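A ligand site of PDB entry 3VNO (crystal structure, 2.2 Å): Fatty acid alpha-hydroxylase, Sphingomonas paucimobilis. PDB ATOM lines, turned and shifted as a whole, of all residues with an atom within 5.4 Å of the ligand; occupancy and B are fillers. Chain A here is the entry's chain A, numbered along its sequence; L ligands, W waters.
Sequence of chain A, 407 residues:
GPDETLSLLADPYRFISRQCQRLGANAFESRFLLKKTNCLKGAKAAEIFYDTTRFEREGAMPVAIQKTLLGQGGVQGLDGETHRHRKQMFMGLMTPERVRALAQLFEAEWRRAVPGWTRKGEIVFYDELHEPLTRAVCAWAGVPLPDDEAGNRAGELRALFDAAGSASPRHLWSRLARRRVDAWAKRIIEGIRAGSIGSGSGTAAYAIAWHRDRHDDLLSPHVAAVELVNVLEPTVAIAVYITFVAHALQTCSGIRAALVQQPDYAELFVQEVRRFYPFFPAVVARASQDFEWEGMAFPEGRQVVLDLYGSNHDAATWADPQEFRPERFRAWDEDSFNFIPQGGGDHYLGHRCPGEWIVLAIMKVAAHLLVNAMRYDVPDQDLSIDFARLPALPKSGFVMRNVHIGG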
ATOM      1  N   PHE A  49      41.776  -9.373 -13.189  1.00  0.00           N
ATOM      2  CA  PHE A  49      41.391  -8.188 -12.416  1.00  0.00           C
ATOM      3  C   PHE A  49      40.124  -8.411 -11.593  1.00  0.00           C
ATOM      4  O   PHE A  49      40.022  -7.942 -10.449  1.00  0.00           O
ATOM      5  CB  PHE A  49      41.193  -6.973 -13.348  1.00  0.00           C
ATOM      6  CG  PHE A  49      41.048  -5.632 -12.606  1.00  0.00           C
ATOM      7  CD1 PHE A  49      42.170  -4.932 -12.158  1.00  0.00           C
ATOM      8  CD2 PHE A  49      39.789  -5.074 -12.400  1.00  0.00           C
ATOM      9  CE1 PHE A  49      42.021  -3.684 -11.497  1.00  0.00           C
ATOM     10  CE2 PHE A  49      39.633  -3.842 -11.747  1.00  0.00           C
ATOM     11  CZ  PHE A  49      40.755  -3.142 -11.299  1.00  0.00           C
ATOM     12  N   TYR A  50      39.179  -9.153 -12.177  1.00  0.00           N
ATOM     13  CA  TYR A  50      37.910  -9.470 -11.533  1.00  0.00           C
ATOM     14  C   TYR A  50      37.940 -10.726 -10.677  1.00  0.00           C
ATOM     15  O   TYR A  50      36.917 -11.134 -10.110  1.00  0.00           O
ATOM     16  CB  TYR A  50      36.771  -9.501 -12.565  1.00  0.00           C
ATOM     17  CG  TYR A  50      36.408  -8.091 -12.941  1.00  0.00           C
ATOM     18  CD1 TYR A  50      35.661  -7.289 -12.050  1.00  0.00           C
ATOM     19  CD2 TYR A  50      36.850  -7.513 -14.134  1.00  0.00           C
ATOM     20  CE1 TYR A  50      35.350  -5.974 -12.355  1.00  0.00           C
ATOM     21  CE2 TYR A  50      36.537  -6.161 -14.440  1.00  0.00           C
ATOM     22  CZ  TYR A  50      35.772  -5.418 -13.557  1.00  0.00           C
ATOM     23  OH  TYR A  50      35.450  -4.083 -13.821  1.00  0.00           O
ATOM     24  N   ARG A  57      39.153  -4.094  -3.388  1.00  0.00           N
ATOM     25  CA  ARG A  57      38.930  -2.668  -3.637  1.00  0.00           C
ATOM     26  C   ARG A  57      39.169  -1.809  -2.406  1.00  0.00           C
ATOM     27  O   ARG A  57      39.359  -0.622  -2.520  1.00  0.00           O
ATOM     28  CB  ARG A  57      37.534  -2.389  -4.185  1.00  0.00           C
ATOM     29  CG  ARG A  57      37.192  -3.208  -5.471  1.00  0.00           C
ATOM     30  CD  ARG A  57      38.241  -3.065  -6.585  1.00  0.00           C
ATOM     31  NE  ARG A  57      37.820  -3.766  -7.787  1.00  0.00           N
ATOM     32  CZ  ARG A  57      36.963  -3.282  -8.686  1.00  0.00           C
ATOM     33  NH1 ARG A  57      36.433  -2.074  -8.536  1.00  0.00           N
ATOM     34  NH2 ARG A  57      36.641  -4.030  -9.739  1.00  0.00           N
ATOM     35  N   VAL A  75      29.214   1.118  -1.855  1.00  0.00           N
ATOM     36  CA  VAL A  75      29.468  -0.244  -2.362  1.00  0.00           C
ATOM     37  C   VAL A  75      30.840  -0.415  -3.073  1.00  0.00           C
ATOM     38  O   VAL A  75      31.429  -1.484  -2.995  1.00  0.00           O
ATOM     39  CB  VAL A  75      28.309  -0.703  -3.267  1.00  0.00           C
ATOM     40  CG1 VAL A  75      28.211   0.152  -4.548  1.00  0.00           C
ATOM     41  CG2 VAL A  75      28.395  -2.209  -3.587  1.00  0.00           C
ATOM     42  N   GLN A  76      31.345   0.641  -3.719  1.00  0.00           N
ATOM     43  CA  GLN A  76      32.632   0.569  -4.477  1.00  0.00           C
ATOM     44  C   GLN A  76      33.861   0.258  -3.600  1.00  0.00           C
ATOM     45  O   GLN A  76      34.842  -0.320  -4.090  1.00  0.00           O
ATOM     46  CB  GLN A  76      32.916   1.884  -5.240  1.00  0.00           C
ATOM     47  CG  GLN A  76      31.871   2.239  -6.312  1.00  0.00           C
ATOM     48  CD  GLN A  76      30.722   3.110  -5.786  1.00  0.00           C
ATOM     49  OE1 GLN A  76      30.491   3.183  -4.573  1.00  0.00           O
ATOM     50  NE2 GLN A  76      30.004   3.766  -6.701  1.00  0.00           N
ATOM     51  N   HIS A  83      30.556  -6.835   0.555  1.00  0.00           N
ATOM     52  CA  HIS A  83      30.282  -6.273  -0.774  1.00  0.00           C
ATOM     53  C   HIS A  83      29.081  -6.983  -1.448  1.00  0.00           C
ATOM     54  O   HIS A  83      28.181  -6.328  -1.962  1.00  0.00           O
ATOM     55  CB  HIS A  83      31.458  -6.471  -1.736  1.00  0.00           C
ATOM     56  CG  HIS A  83      31.099  -6.077  -3.134  1.00  0.00           C
ATOM     57  ND1 HIS A  83      30.761  -6.995  -4.096  1.00  0.00           N
ATOM     58  CD2 HIS A  83      30.893  -4.851  -3.682  1.00  0.00           C
ATOM     59  CE1 HIS A  83      30.422  -6.364  -5.206  1.00  0.00           C
ATOM     60  NE2 HIS A  83      30.487  -5.063  -4.983  1.00  0.00           N
ATOM     61  N   LYS A  87      25.819  -5.223  -2.790  1.00  0.00           N
ATOM     62  CA  LYS A  87      25.592  -5.195  -4.235  1.00  0.00           C
ATOM     63  C   LYS A  87      24.202  -5.739  -4.594  1.00  0.00           C
ATOM     64  O   LYS A  87      23.559  -5.245  -5.523  1.00  0.00           O
ATOM     65  CB  LYS A  87      26.675  -6.004  -4.970  1.00  0.00           C
ATOM     66  CG  LYS A  87      26.577  -6.001  -6.515  1.00  0.00           C
ATOM     67  CD  LYS A  87      26.601  -4.549  -7.107  1.00  0.00           C
ATOM     68  CE  LYS A  87      26.902  -4.583  -8.618  1.00  0.00           C
ATOM     69  NZ  LYS A  87      28.359  -4.847  -8.852  1.00  0.00           N
ATOM     70  N   PHE A  90      21.535  -3.129  -4.836  1.00  0.00           N
ATOM     71  CA  PHE A  90      21.440  -2.433  -6.119  1.00  0.00           C
ATOM     72  C   PHE A  90      20.820  -3.313  -7.207  1.00  0.00           C
ATOM     73  O   PHE A  90      20.003  -2.833  -7.987  1.00  0.00           O
ATOM     74  CB  PHE A  90      22.800  -1.930  -6.564  1.00  0.00           C
ATOM     75  CG  PHE A  90      23.329  -0.766  -5.746  1.00  0.00           C
ATOM     76  CD1 PHE A  90      22.994   0.549  -6.080  1.00  0.00           C
ATOM     77  CD2 PHE A  90      24.175  -0.978  -4.650  1.00  0.00           C
ATOM     78  CE1 PHE A  90      23.501   1.645  -5.347  1.00  0.00           C
ATOM     79  CE2 PHE A  90      24.696   0.105  -3.904  1.00  0.00           C
ATOM     80  CZ  PHE A  90      24.363   1.415  -4.255  1.00  0.00           C
ATOM     81  N   MET A  94      16.883  -3.510 -10.426  1.00  0.00           N
ATOM     82  CA  MET A  94      17.042  -3.558 -11.893  1.00  0.00           C
ATOM     83  C   MET A  94      16.197  -4.631 -12.590  1.00  0.00           C
ATOM     84  O   MET A  94      16.686  -5.350 -13.478  1.00  0.00           O
ATOM     85  CB  MET A  94      18.524  -3.755 -12.239  1.00  0.00           C
ATOM     86  CG  MET A  94      19.491  -2.828 -11.485  1.00  0.00           C
ATOM     87  SD  MET A  94      18.982  -1.107 -11.688  1.00  0.00           S
ATOM     88  CE  MET A  94      20.265  -0.241 -10.795  1.00  0.00           C
ATOM     89  N   ASN A 230      24.600   7.055  -5.399  1.00  0.00           N
ATOM     90  CA  ASN A 230      25.137   6.065  -6.324  1.00  0.00           C
ATOM     91  C   ASN A 230      24.069   5.577  -7.357  1.00  0.00           C
ATOM     92  O   ASN A 230      24.438   4.917  -8.296  1.00  0.00           O
ATOM     93  CB  ASN A 230      25.691   4.840  -5.571  1.00  0.00           C
ATOM     94  CG  ASN A 230      27.184   4.946  -5.283  1.00  0.00           C
ATOM     95  OD1 ASN A 230      27.953   5.551  -6.031  1.00  0.00           O
ATOM     96  ND2 ASN A 230      27.617   4.314  -4.188  1.00  0.00           N
ATOM     97  N   VAL A 231      22.780   5.899  -7.158  1.00  0.00           N
ATOM     98  CA  VAL A 231      21.747   5.675  -8.194  1.00  0.00           C
ATOM     99  C   VAL A 231      21.481   6.982  -8.976  1.00  0.00           C
ATOM    100  O   VAL A 231      21.398   6.980 -10.202  1.00  0.00           O
ATOM    101  CB  VAL A 231      20.400   5.188  -7.573  1.00  0.00           C
ATOM    102  CG1 VAL A 231      19.286   5.104  -8.645  1.00  0.00           C
ATOM    103  CG2 VAL A 231      20.572   3.798  -6.852  1.00  0.00           C
ATOM    104  N   PRO A 234      24.983   8.580 -11.243  1.00  0.00           N
ATOM    105  CA  PRO A 234      25.383   7.992 -12.508  1.00  0.00           C
ATOM    106  C   PRO A 234      24.231   7.955 -13.516  1.00  0.00           C
ATOM    107  O   PRO A 234      24.505   7.939 -14.716  1.00  0.00           O
ATOM    108  CB  PRO A 234      25.836   6.573 -12.126  1.00  0.00           C
ATOM    109  CG  PRO A 234      25.154   6.305 -10.818  1.00  0.00           C
ATOM    110  CD  PRO A 234      25.062   7.618 -10.120  1.00  0.00           C
ATOM    111  N   THR A 235      22.978   7.992 -13.067  1.00  0.00           N
ATOM    112  CA  THR A 235      21.875   8.119 -14.035  1.00  0.00           C
ATOM    113  C   THR A 235      21.926   9.447 -14.772  1.00  0.00           C
ATOM    114  O   THR A 235      21.756   9.499 -16.000  1.00  0.00           O
ATOM    115  CB  THR A 235      20.496   7.885 -13.381  1.00  0.00           C
ATOM    116  OG1 THR A 235      20.486   6.587 -12.770  1.00  0.00           O
ATOM    117  CG2 THR A 235      19.375   7.951 -14.430  1.00  0.00           C
ATOM    118  N   ALA A 237      24.616  11.068 -15.282  1.00  0.00           N
ATOM    119  CA  ALA A 237      25.819  10.943 -16.146  1.00  0.00           C
ATOM    120  C   ALA A 237      25.535  10.303 -17.531  1.00  0.00           C
ATOM    121  O   ALA A 237      26.366  10.392 -18.448  1.00  0.00           O
ATOM    122  CB  ALA A 237      26.951  10.189 -15.408  1.00  0.00           C
ATOM    123  N   ILE A 238      24.362   9.692 -17.691  1.00  0.00           N
ATOM    124  CA  ILE A 238      23.963   9.146 -19.009  1.00  0.00           C
ATOM    125  C   ILE A 238      23.875  10.277 -20.048  1.00  0.00           C
ATOM    126  O   ILE A 238      23.835  10.014 -21.254  1.00  0.00           O
ATOM    127  CB  ILE A 238      22.664   8.315 -18.918  1.00  0.00           C
ATOM    128  CG1 ILE A 238      22.851   7.140 -17.934  1.00  0.00           C
ATOM    129  CG2 ILE A 238      22.278   7.710 -20.300  1.00  0.00           C
ATOM    130  CD1 ILE A 238      21.556   6.496 -17.487  1.00  0.00           C
ATOM    131  N   TYR A 241      26.615   9.759 -22.594  1.00  0.00           N
ATOM    132  CA  TYR A 241      26.307   8.762 -23.648  1.00  0.00           C
ATOM    133  C   TYR A 241      25.248   9.247 -24.623  1.00  0.00           C
ATOM    134  O   TYR A 241      25.322   8.922 -25.815  1.00  0.00           O
ATOM    135  CB  TYR A 241      25.859   7.400 -23.075  1.00  0.00           C
ATOM    136  CG  TYR A 241      26.984   6.432 -22.758  1.00  0.00           C
ATOM    137  CD1 TYR A 241      28.088   6.286 -23.632  1.00  0.00           C
ATOM    138  CD2 TYR A 241      26.918   5.613 -21.615  1.00  0.00           C
ATOM    139  CE1 TYR A 241      29.127   5.385 -23.346  1.00  0.00           C
ATOM    140  CE2 TYR A 241      27.937   4.691 -21.337  1.00  0.00           C
ATOM    141  CZ  TYR A 241      29.045   4.585 -22.199  1.00  0.00           C
ATOM    142  OH  TYR A 241      30.047   3.699 -21.906  1.00  0.00           O
ATOM    143  N   PHE A 279      34.436   6.975 -22.008  1.00  0.00           N
ATOM    144  CA  PHE A 279      33.619   7.507 -20.914  1.00  0.00           C
ATOM    145  C   PHE A 279      34.335   7.284 -19.571  1.00  0.00           C
ATOM    146  O   PHE A 279      34.909   8.222 -19.003  1.00  0.00           O
ATOM    147  CB  PHE A 279      32.194   6.915 -20.943  1.00  0.00           C
ATOM    148  CG  PHE A 279      31.183   7.652 -20.054  1.00  0.00           C
ATOM    149  CD1 PHE A 279      31.583   8.399 -18.951  1.00  0.00           C
ATOM    150  CD2 PHE A 279      29.821   7.550 -20.328  1.00  0.00           C
ATOM    151  CE1 PHE A 279      30.629   9.046 -18.134  1.00  0.00           C
ATOM    152  CE2 PHE A 279      28.862   8.208 -19.528  1.00  0.00           C
ATOM    153  CZ  PHE A 279      29.253   8.943 -18.441  1.00  0.00           C
ATOM    154  N   PHE A 280      34.295   6.052 -19.067  1.00  0.00           N
ATOM    155  CA  PHE A 280      35.025   5.687 -17.865  1.00  0.00           C
ATOM    156  C   PHE A 280      36.408   5.182 -18.253  1.00  0.00           C
ATOM    157  O   PHE A 280      36.514   4.175 -18.946  1.00  0.00           O
ATOM    158  CB  PHE A 280      34.259   4.619 -17.091  1.00  0.00           C
ATOM    159  CG  PHE A 280      34.531   4.645 -15.626  1.00  0.00           C
ATOM    160  CD1 PHE A 280      35.760   4.224 -15.119  1.00  0.00           C
ATOM    161  CD2 PHE A 280      33.564   5.102 -14.754  1.00  0.00           C
ATOM    162  CE1 PHE A 280      36.024   4.269 -13.760  1.00  0.00           C
ATOM    163  CE2 PHE A 280      33.811   5.134 -13.375  1.00  0.00           C
ATOM    164  CZ  PHE A 280      35.055   4.714 -12.884  1.00  0.00           C
ATOM    165  N   VAL A 283      39.645   1.394 -14.025  1.00  0.00           N
ATOM    166  CA  VAL A 283      39.196   1.012 -12.708  1.00  0.00           C
ATOM    167  C   VAL A 283      40.423   0.589 -11.923  1.00  0.00           C
ATOM    168  O   VAL A 283      41.386   0.103 -12.509  1.00  0.00           O
ATOM    169  CB  VAL A 283      38.173  -0.159 -12.785  1.00  0.00           C
ATOM    170  CG1 VAL A 283      37.868  -0.734 -11.411  1.00  0.00           C
ATOM    171  CG2 VAL A 283      36.878   0.343 -13.442  1.00  0.00           C
ATOM    172  N   LEU A 308      39.895   0.377 -19.343  1.00  0.00           N
ATOM    173  CA  LEU A 308      38.627   0.012 -19.988  1.00  0.00           C
ATOM    174  C   LEU A 308      38.588   0.440 -21.443  1.00  0.00           C
ATOM    175  O   LEU A 308      38.186  -0.342 -22.301  1.00  0.00           O
ATOM    176  CB  LEU A 308      37.418   0.604 -19.231  1.00  0.00           C
ATOM    177  CG  LEU A 308      37.280   0.255 -17.739  1.00  0.00           C
ATOM    178  CD1 LEU A 308      36.026   0.913 -17.122  1.00  0.00           C
ATOM    179  CD2 LEU A 308      37.276  -1.270 -17.464  1.00  0.00           C
ATOM    180  N   PRO A 341      32.794  -1.445 -20.964  1.00  0.00           N
ATOM    181  CA  PRO A 341      32.677   0.012 -20.811  1.00  0.00           C
ATOM    182  C   PRO A 341      32.232   0.410 -19.384  1.00  0.00           C
ATOM    183  O   PRO A 341      32.476   1.556 -18.945  1.00  0.00           O
ATOM    184  CB  PRO A 341      31.608   0.402 -21.830  1.00  0.00           C
ATOM    185  CG  PRO A 341      30.782  -0.838 -22.006  1.00  0.00           C
ATOM    186  CD  PRO A 341      31.786  -1.962 -21.923  1.00  0.00           C
ATOM    187  N   GLN A 342      31.619  -0.517 -18.675  1.00  0.00           N
ATOM    188  CA  GLN A 342      31.105  -0.254 -17.325  1.00  0.00           C
ATOM    189  C   GLN A 342      31.520  -1.401 -16.400  1.00  0.00           C
ATOM    190  O   GLN A 342      30.774  -1.807 -15.487  1.00  0.00           O
ATOM    191  CB  GLN A 342      29.584  -0.083 -17.409  1.00  0.00           C
ATOM    192  CG  GLN A 342      29.175   1.066 -18.371  1.00  0.00           C
ATOM    193  CD  GLN A 342      27.685   1.369 -18.309  1.00  0.00           C
ATOM    194  OE1 GLN A 342      27.035   1.526 -19.336  1.00  0.00           O
ATOM    195  NE2 GLN A 342      27.136   1.422 -17.092  1.00  0.00           N
ATOM    196  N   GLY A 343      32.728  -1.914 -16.647  1.00  0.00           N
ATOM    197  CA  GLY A 343      33.276  -3.009 -15.884  1.00  0.00           C
ATOM    198  C   GLY A 343      33.038  -4.365 -16.517  1.00  0.00           C
ATOM    199  O   GLY A 343      32.249  -4.513 -17.452  1.00  0.00           O
ATOM    200  N   GLY A 344      33.768  -5.341 -15.997  1.00  0.00           N
ATOM    201  CA  GLY A 344      33.668  -6.714 -16.460  1.00  0.00           C
ATOM    202  C   GLY A 344      33.243  -7.649 -15.349  1.00  0.00           C
ATOM    203  O   GLY A 344      32.947  -7.199 -14.198  1.00  0.00           O
ATOM    204  N   GLY A 350      31.074  -9.377  -8.318  1.00  0.00           N
ATOM    205  CA  GLY A 350      32.153  -8.407  -8.454  1.00  0.00           C
ATOM    206  C   GLY A 350      31.593  -7.014  -8.580  1.00  0.00           C
ATOM    207  O   GLY A 350      30.404  -6.824  -8.406  1.00  0.00           O
ATOM    208  N   HIS A 351      32.441  -6.047  -8.906  1.00  0.00           N
ATOM    209  CA  HIS A 351      32.044  -4.639  -8.875  1.00  0.00           C
ATOM    210  C   HIS A 351      31.454  -4.102 -10.192  1.00  0.00           C
ATOM    211  O   HIS A 351      31.266  -2.888 -10.339  1.00  0.00           O
ATOM    212  CB  HIS A 351      33.246  -3.793  -8.432  1.00  0.00           C
ATOM    213  CG  HIS A 351      33.591  -3.989  -6.980  1.00  0.00           C
ATOM    214  ND1 HIS A 351      33.117  -3.154  -5.999  1.00  0.00           N
ATOM    215  CD2 HIS A 351      34.265  -4.983  -6.346  1.00  0.00           C
ATOM    216  CE1 HIS A 351      33.542  -3.585  -4.813  1.00  0.00           C
ATOM    217  NE2 HIS A 351      34.236  -4.692  -5.007  1.00  0.00           N
ATOM    218  N   ARG A 352      31.186  -5.002 -11.136  1.00  0.00           N
ATOM    219  CA  ARG A 352      30.614  -4.622 -12.447  1.00  0.00           C
ATOM    220  C   ARG A 352      29.444  -3.683 -12.187  1.00  0.00           C
ATOM    221  O   ARG A 352      28.634  -3.935 -11.305  1.00  0.00           O
ATOM    222  CB  ARG A 352      30.145  -5.866 -13.235  1.00  0.00           C
ATOM    223  CG  ARG A 352      29.797  -5.525 -14.705  1.00  0.00           C
ATOM    224  CD  ARG A 352      29.487  -6.741 -15.556  1.00  0.00           C
ATOM    225  NE  ARG A 352      29.100  -6.372 -16.926  1.00  0.00           N
ATOM    226  CZ  ARG A 352      29.631  -6.909 -18.027  1.00  0.00           C
ATOM    227  NH1 ARG A 352      30.550  -7.882 -17.946  1.00  0.00           N
ATOM    228  NH2 ARG A 352      29.231  -6.480 -19.209  1.00  0.00           N
ATOM    229  N   CYS A 353      29.347  -2.622 -12.977  1.00  0.00           N
ATOM    230  CA  CYS A 353      28.222  -1.678 -12.897  1.00  0.00           C
ATOM    231  C   CYS A 353      26.828  -2.301 -12.941  1.00  0.00           C
ATOM    232  O   CYS A 353      26.476  -2.971 -13.901  1.00  0.00           O
ATOM    233  CB  CYS A 353      28.338  -0.716 -14.062  1.00  0.00           C
ATOM    234  SG  CYS A 353      27.125   0.587 -14.012  1.00  0.00           S
ATOM    235  N   PRO A 354      26.003  -2.035 -11.914  1.00  0.00           N
ATOM    236  CA  PRO A 354      24.633  -2.544 -11.942  1.00  0.00           C
ATOM    237  C   PRO A 354      23.725  -1.631 -12.778  1.00  0.00           C
ATOM    238  O   PRO A 354      22.567  -1.988 -13.026  1.00  0.00           O
ATOM    239  CB  PRO A 354      24.215  -2.458 -10.475  1.00  0.00           C
ATOM    240  CG  PRO A 354      24.910  -1.210 -10.015  1.00  0.00           C
ATOM    241  CD  PRO A 354      26.294  -1.343 -10.644  1.00  0.00           C
ATOM    242  N   GLY A 355      24.256  -0.469 -13.172  1.00  0.00           N
ATOM    243  CA  GLY A 355      23.517   0.466 -14.018  1.00  0.00           C
ATOM    244  C   GLY A 355      23.393   0.171 -15.523  1.00  0.00           C
ATOM    245  O   GLY A 355      22.766   0.963 -16.234  1.00  0.00           O
ATOM    246  N   GLU A 356      23.970  -0.945 -16.004  1.00  0.00           N
ATOM    247  CA  GLU A 356      24.004  -1.197 -17.454  1.00  0.00           C
ATOM    248  C   GLU A 356      22.611  -1.307 -18.076  1.00  0.00           C
ATOM    249  O   GLU A 356      22.393  -0.804 -19.167  1.00  0.00           O
ATOM    250  CB  GLU A 356      24.851  -2.459 -17.824  1.00  0.00           C
ATOM    251  CG  GLU A 356      26.336  -2.255 -17.533  1.00  0.00           C
ATOM    252  CD  GLU A 356      27.183  -3.416 -17.962  1.00  0.00           C
ATOM    253  OE1 GLU A 356      27.078  -4.478 -17.322  1.00  0.00           O
ATOM    254  OE2 GLU A 356      27.959  -3.258 -18.941  1.00  0.00           O
ATOM    255  N   ILE A 358      19.856   0.161 -17.211  1.00  0.00           N
ATOM    256  CA  ILE A 358      19.337   1.517 -17.275  1.00  0.00           C
ATOM    257  C   ILE A 358      20.024   2.306 -18.393  1.00  0.00           C
ATOM    258  O   ILE A 358      19.360   2.976 -19.194  1.00  0.00           O
ATOM    259  CB  ILE A 358      19.518   2.243 -15.892  1.00  0.00           C
ATOM    260  CG1 ILE A 358      18.532   1.664 -14.862  1.00  0.00           C
ATOM    261  CG2 ILE A 358      19.421   3.799 -16.034  1.00  0.00           C
ATOM    262  CD1 ILE A 358      18.836   2.124 -13.377  1.00  0.00           C
ATOM    263  N   VAL A 359      21.343   2.236 -18.444  1.00  0.00           N
ATOM    264  CA  VAL A 359      22.092   2.941 -19.476  1.00  0.00           C
ATOM    265  C   VAL A 359      21.612   2.521 -20.874  1.00  0.00           C
ATOM    266  O   VAL A 359      21.372   3.388 -21.720  1.00  0.00           O
ATOM    267  CB  VAL A 359      23.625   2.693 -19.371  1.00  0.00           C
ATOM    268  CG1 VAL A 359      24.343   3.201 -20.612  1.00  0.00           C
ATOM    269  CG2 VAL A 359      24.186   3.344 -18.129  1.00  0.00           C
HETATM  270  C1  LIG L   1      30.226   0.826 -11.005  1.00  0.00           C
HETATM  271  C2  LIG L   1      30.634   2.827 -15.420  1.00  0.00           C
HETATM  272  C3  LIG L   1      26.001   4.221 -15.151  1.00  0.00           C
HETATM  273  C4  LIG L   1      25.688   2.584 -10.632  1.00  0.00           C
HETATM  274  C5  LIG L   1      30.723   1.219 -12.219  1.00  0.00           C
HETATM  275  C6  LIG L   1      32.072   0.958 -12.700  1.00  0.00           C
HETATM  276  C7  LIG L   1      32.171   1.504 -13.939  1.00  0.00           C
HETATM  277  C8  LIG L   1      30.922   2.135 -14.261  1.00  0.00           C
HETATM  278  C9  LIG L   1      33.406   1.513 -14.861  1.00  0.00           C
HETATM  279  C10 LIG L   1      33.149   0.219 -11.865  1.00  0.00           C
HETATM  280  C11 LIG L   1      33.272  -1.301 -12.095  1.00  0.00           C
HETATM  281  C12 LIG L   1      34.379  -1.853 -11.200  1.00  0.00           C
HETATM  282  O1  LIG L   1      34.937  -2.949 -11.530  1.00  0.00           O
HETATM  283  O2  LIG L   1      34.700  -1.220 -10.133  1.00  0.00           O
HETATM  284  C13 LIG L   1      29.439   3.490 -15.689  1.00  0.00           C
HETATM  285  C14 LIG L   1      29.194   4.407 -16.781  1.00  0.00           C
HETATM  286  C15 LIG L   1      27.916   4.808 -16.704  1.00  0.00           C
HETATM  287  C16 LIG L   1      27.311   4.160 -15.557  1.00  0.00           C
HETATM  288  C17 LIG L   1      30.219   4.819 -17.854  1.00  0.00           C
HETATM  289  C18 LIG L   1      27.227   5.788 -17.693  1.00  0.00           C
HETATM  290  C19 LIG L   1      26.451   6.780 -17.233  1.00  0.00           C
HETATM  291  C20 LIG L   1      25.462   3.782 -13.977  1.00  0.00           C
HETATM  292  C21 LIG L   1      24.071   3.901 -13.585  1.00  0.00           C
HETATM  293  C22 LIG L   1      23.954   3.442 -12.336  1.00  0.00           C
HETATM  294  C23 LIG L   1      25.289   3.045 -11.880  1.00  0.00           C
HETATM  295  C24 LIG L   1      22.907   4.440 -14.448  1.00  0.00           C
HETATM  296  C25 LIG L   1      22.577   3.459 -11.623  1.00  0.00           C
HETATM  297  C26 LIG L   1      22.200   2.542 -10.744  1.00  0.00           C
HETATM  298  C27 LIG L   1      26.895   2.043 -10.279  1.00  0.00           C
HETATM  299  C28 LIG L   1      27.216   1.547  -8.959  1.00  0.00           C
HETATM  300  C29 LIG L   1      28.613   0.958  -9.088  1.00  0.00           C
HETATM  301  C30 LIG L   1      29.021   1.212 -10.449  1.00  0.00           C
HETATM  302  C31 LIG L   1      26.328   1.558  -7.697  1.00  0.00           C
HETATM  303  C32 LIG L   1      29.433   0.282  -7.983  1.00  0.00           C
HETATM  304  C33 LIG L   1      29.131  -1.215  -8.068  1.00  0.00           C
HETATM  305  C34 LIG L   1      30.068  -2.057  -7.208  1.00  0.00           C
HETATM  306  O3  LIG L   1      29.771  -3.267  -6.994  1.00  0.00           O
HETATM  307  O4  LIG L   1      31.100  -1.518  -6.715  1.00  0.00           O
HETATM  308  N1  LIG L   1      30.055   1.904 -13.216  1.00  0.00           N
HETATM  309  N2  LIG L   1      28.264   3.339 -14.980  1.00  0.00           N
HETATM  310  N3  LIG L   1      26.148   3.228 -12.916  1.00  0.00           N
HETATM  311  N4  LIG L   1      27.968   1.813 -11.124  1.00  0.00           N
HETATM  312 FE1  LIG L   1      28.080   2.511 -13.082  1.00  0.00          FE
HETATM  313  O   HOH W   1      33.094  -0.010  -8.274  1.00  0.00           O
HETATM  314  O   HOH W   2      29.203   4.740 -11.876  1.00  0.00           O
HETATM  315  O   HOH W   3      35.414   1.830  -9.391  1.00  0.00           O
HETATM  316  O   HOH W   4      31.036   3.899 -10.009  1.00  0.00           O
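OG1 of Thr 235 lies within hydrogen-bond range of O of Val 231, at 2.8 Å. The side-chain sulfur (SG) of Cys 353 lies close to the backbone NH (N) of Gly 355 (3.2 Å). The side-chain amino group (NZ) of Lys 87 lies within hydrogen-bond range of the backbone carbonyl oxygen (O) of Gly 350 (2.9 Å). The backbone NH (N) of Cys 353 lies within hydrogen-bond range of the backbone carbonyl oxygen (O) of Gln 342, at 3.0 Å. The side-chain amino group (NZ) of Lys 87 is in hydrogen-bond range of the backbone carbonyl oxygen (O) of Arg 352, 2.6 Å away. A ring nitrogen (ND1) of His 351 lies close to a ring nitrogen (NE2) of His 83 (3.4 Å). The side-chain hydroxyl (OH) of Tyr 50 sits at hydrogen-bond distance from the backbone NH (N) of Gly 344 (3.0 Å). NE2 of Gln 76 sits at hydrogen-bond distance from OD1 of Asn 230 (2.8 Å).
A ring nitrogen (NE2) of His 83 is in hydrogen-bond range of an oxygen (O3) of the ligand, 2.8 Å away. The guanidinium group (NH1) of Arg 57 is in salt-bridge range of an oxygen (O2) of the ligand, 2.5 Å away. The side-chain sulfur (SG) of Cys 353 is bound to an iron atom (FE1) of the ligand (2.3 Å). O1 of the ligand is in hydrogen-bond range of OH of Tyr 50. The side-chain amino group (NZ) of Lys 87 lies within salt-bridge range of an oxygen (O3) of the ligand (2.8 Å). An oxygen (O4) of the ligand sits at hydrogen-bond distance from a ring nitrogen (ND1) of His 351, at 2.7 Å.
NE2 of Gln 342 lies close to N2 of the ligand (3.1 Å). Merely in contact with the ligand: Pro 234 (3.4 Å), Met 94 (3.4 Å), Phe 280 (3.4 Å), Gln 76 (3.4 Å), Gly 355 (3.4 Å), Phe 279 (3.4 Å), Val 283 (3.5 Å), Pro 354 (3.5 Å), Leu 308 (3.5 Å), Asn 230 (3.5 Å), Val 359 (3.6 Å), Ile 238 (3.6 Å), Thr 235 (3.6 Å), Val 75 (3.6 Å), Ala 237 (3.7 Å), Phe 90 (3.7 Å), Tyr 241 (3.9 Å), Gly 350 (3.9 Å), Ile 358 (3.9 Å), Gly 343 (3.9 Å) and Val 231 (3.98 Å). Hydrophobic or aromatic side chains within 4 Å of the ligand: Tyr 50, Val 75, His 83, Phe 90, Met 94, Pro 234, Ala 237, Ile 238, Tyr 241, Phe 279, Phe 280, Val 283, Leu 308, His 351, Pro 354, Ile 358 and Val 359.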
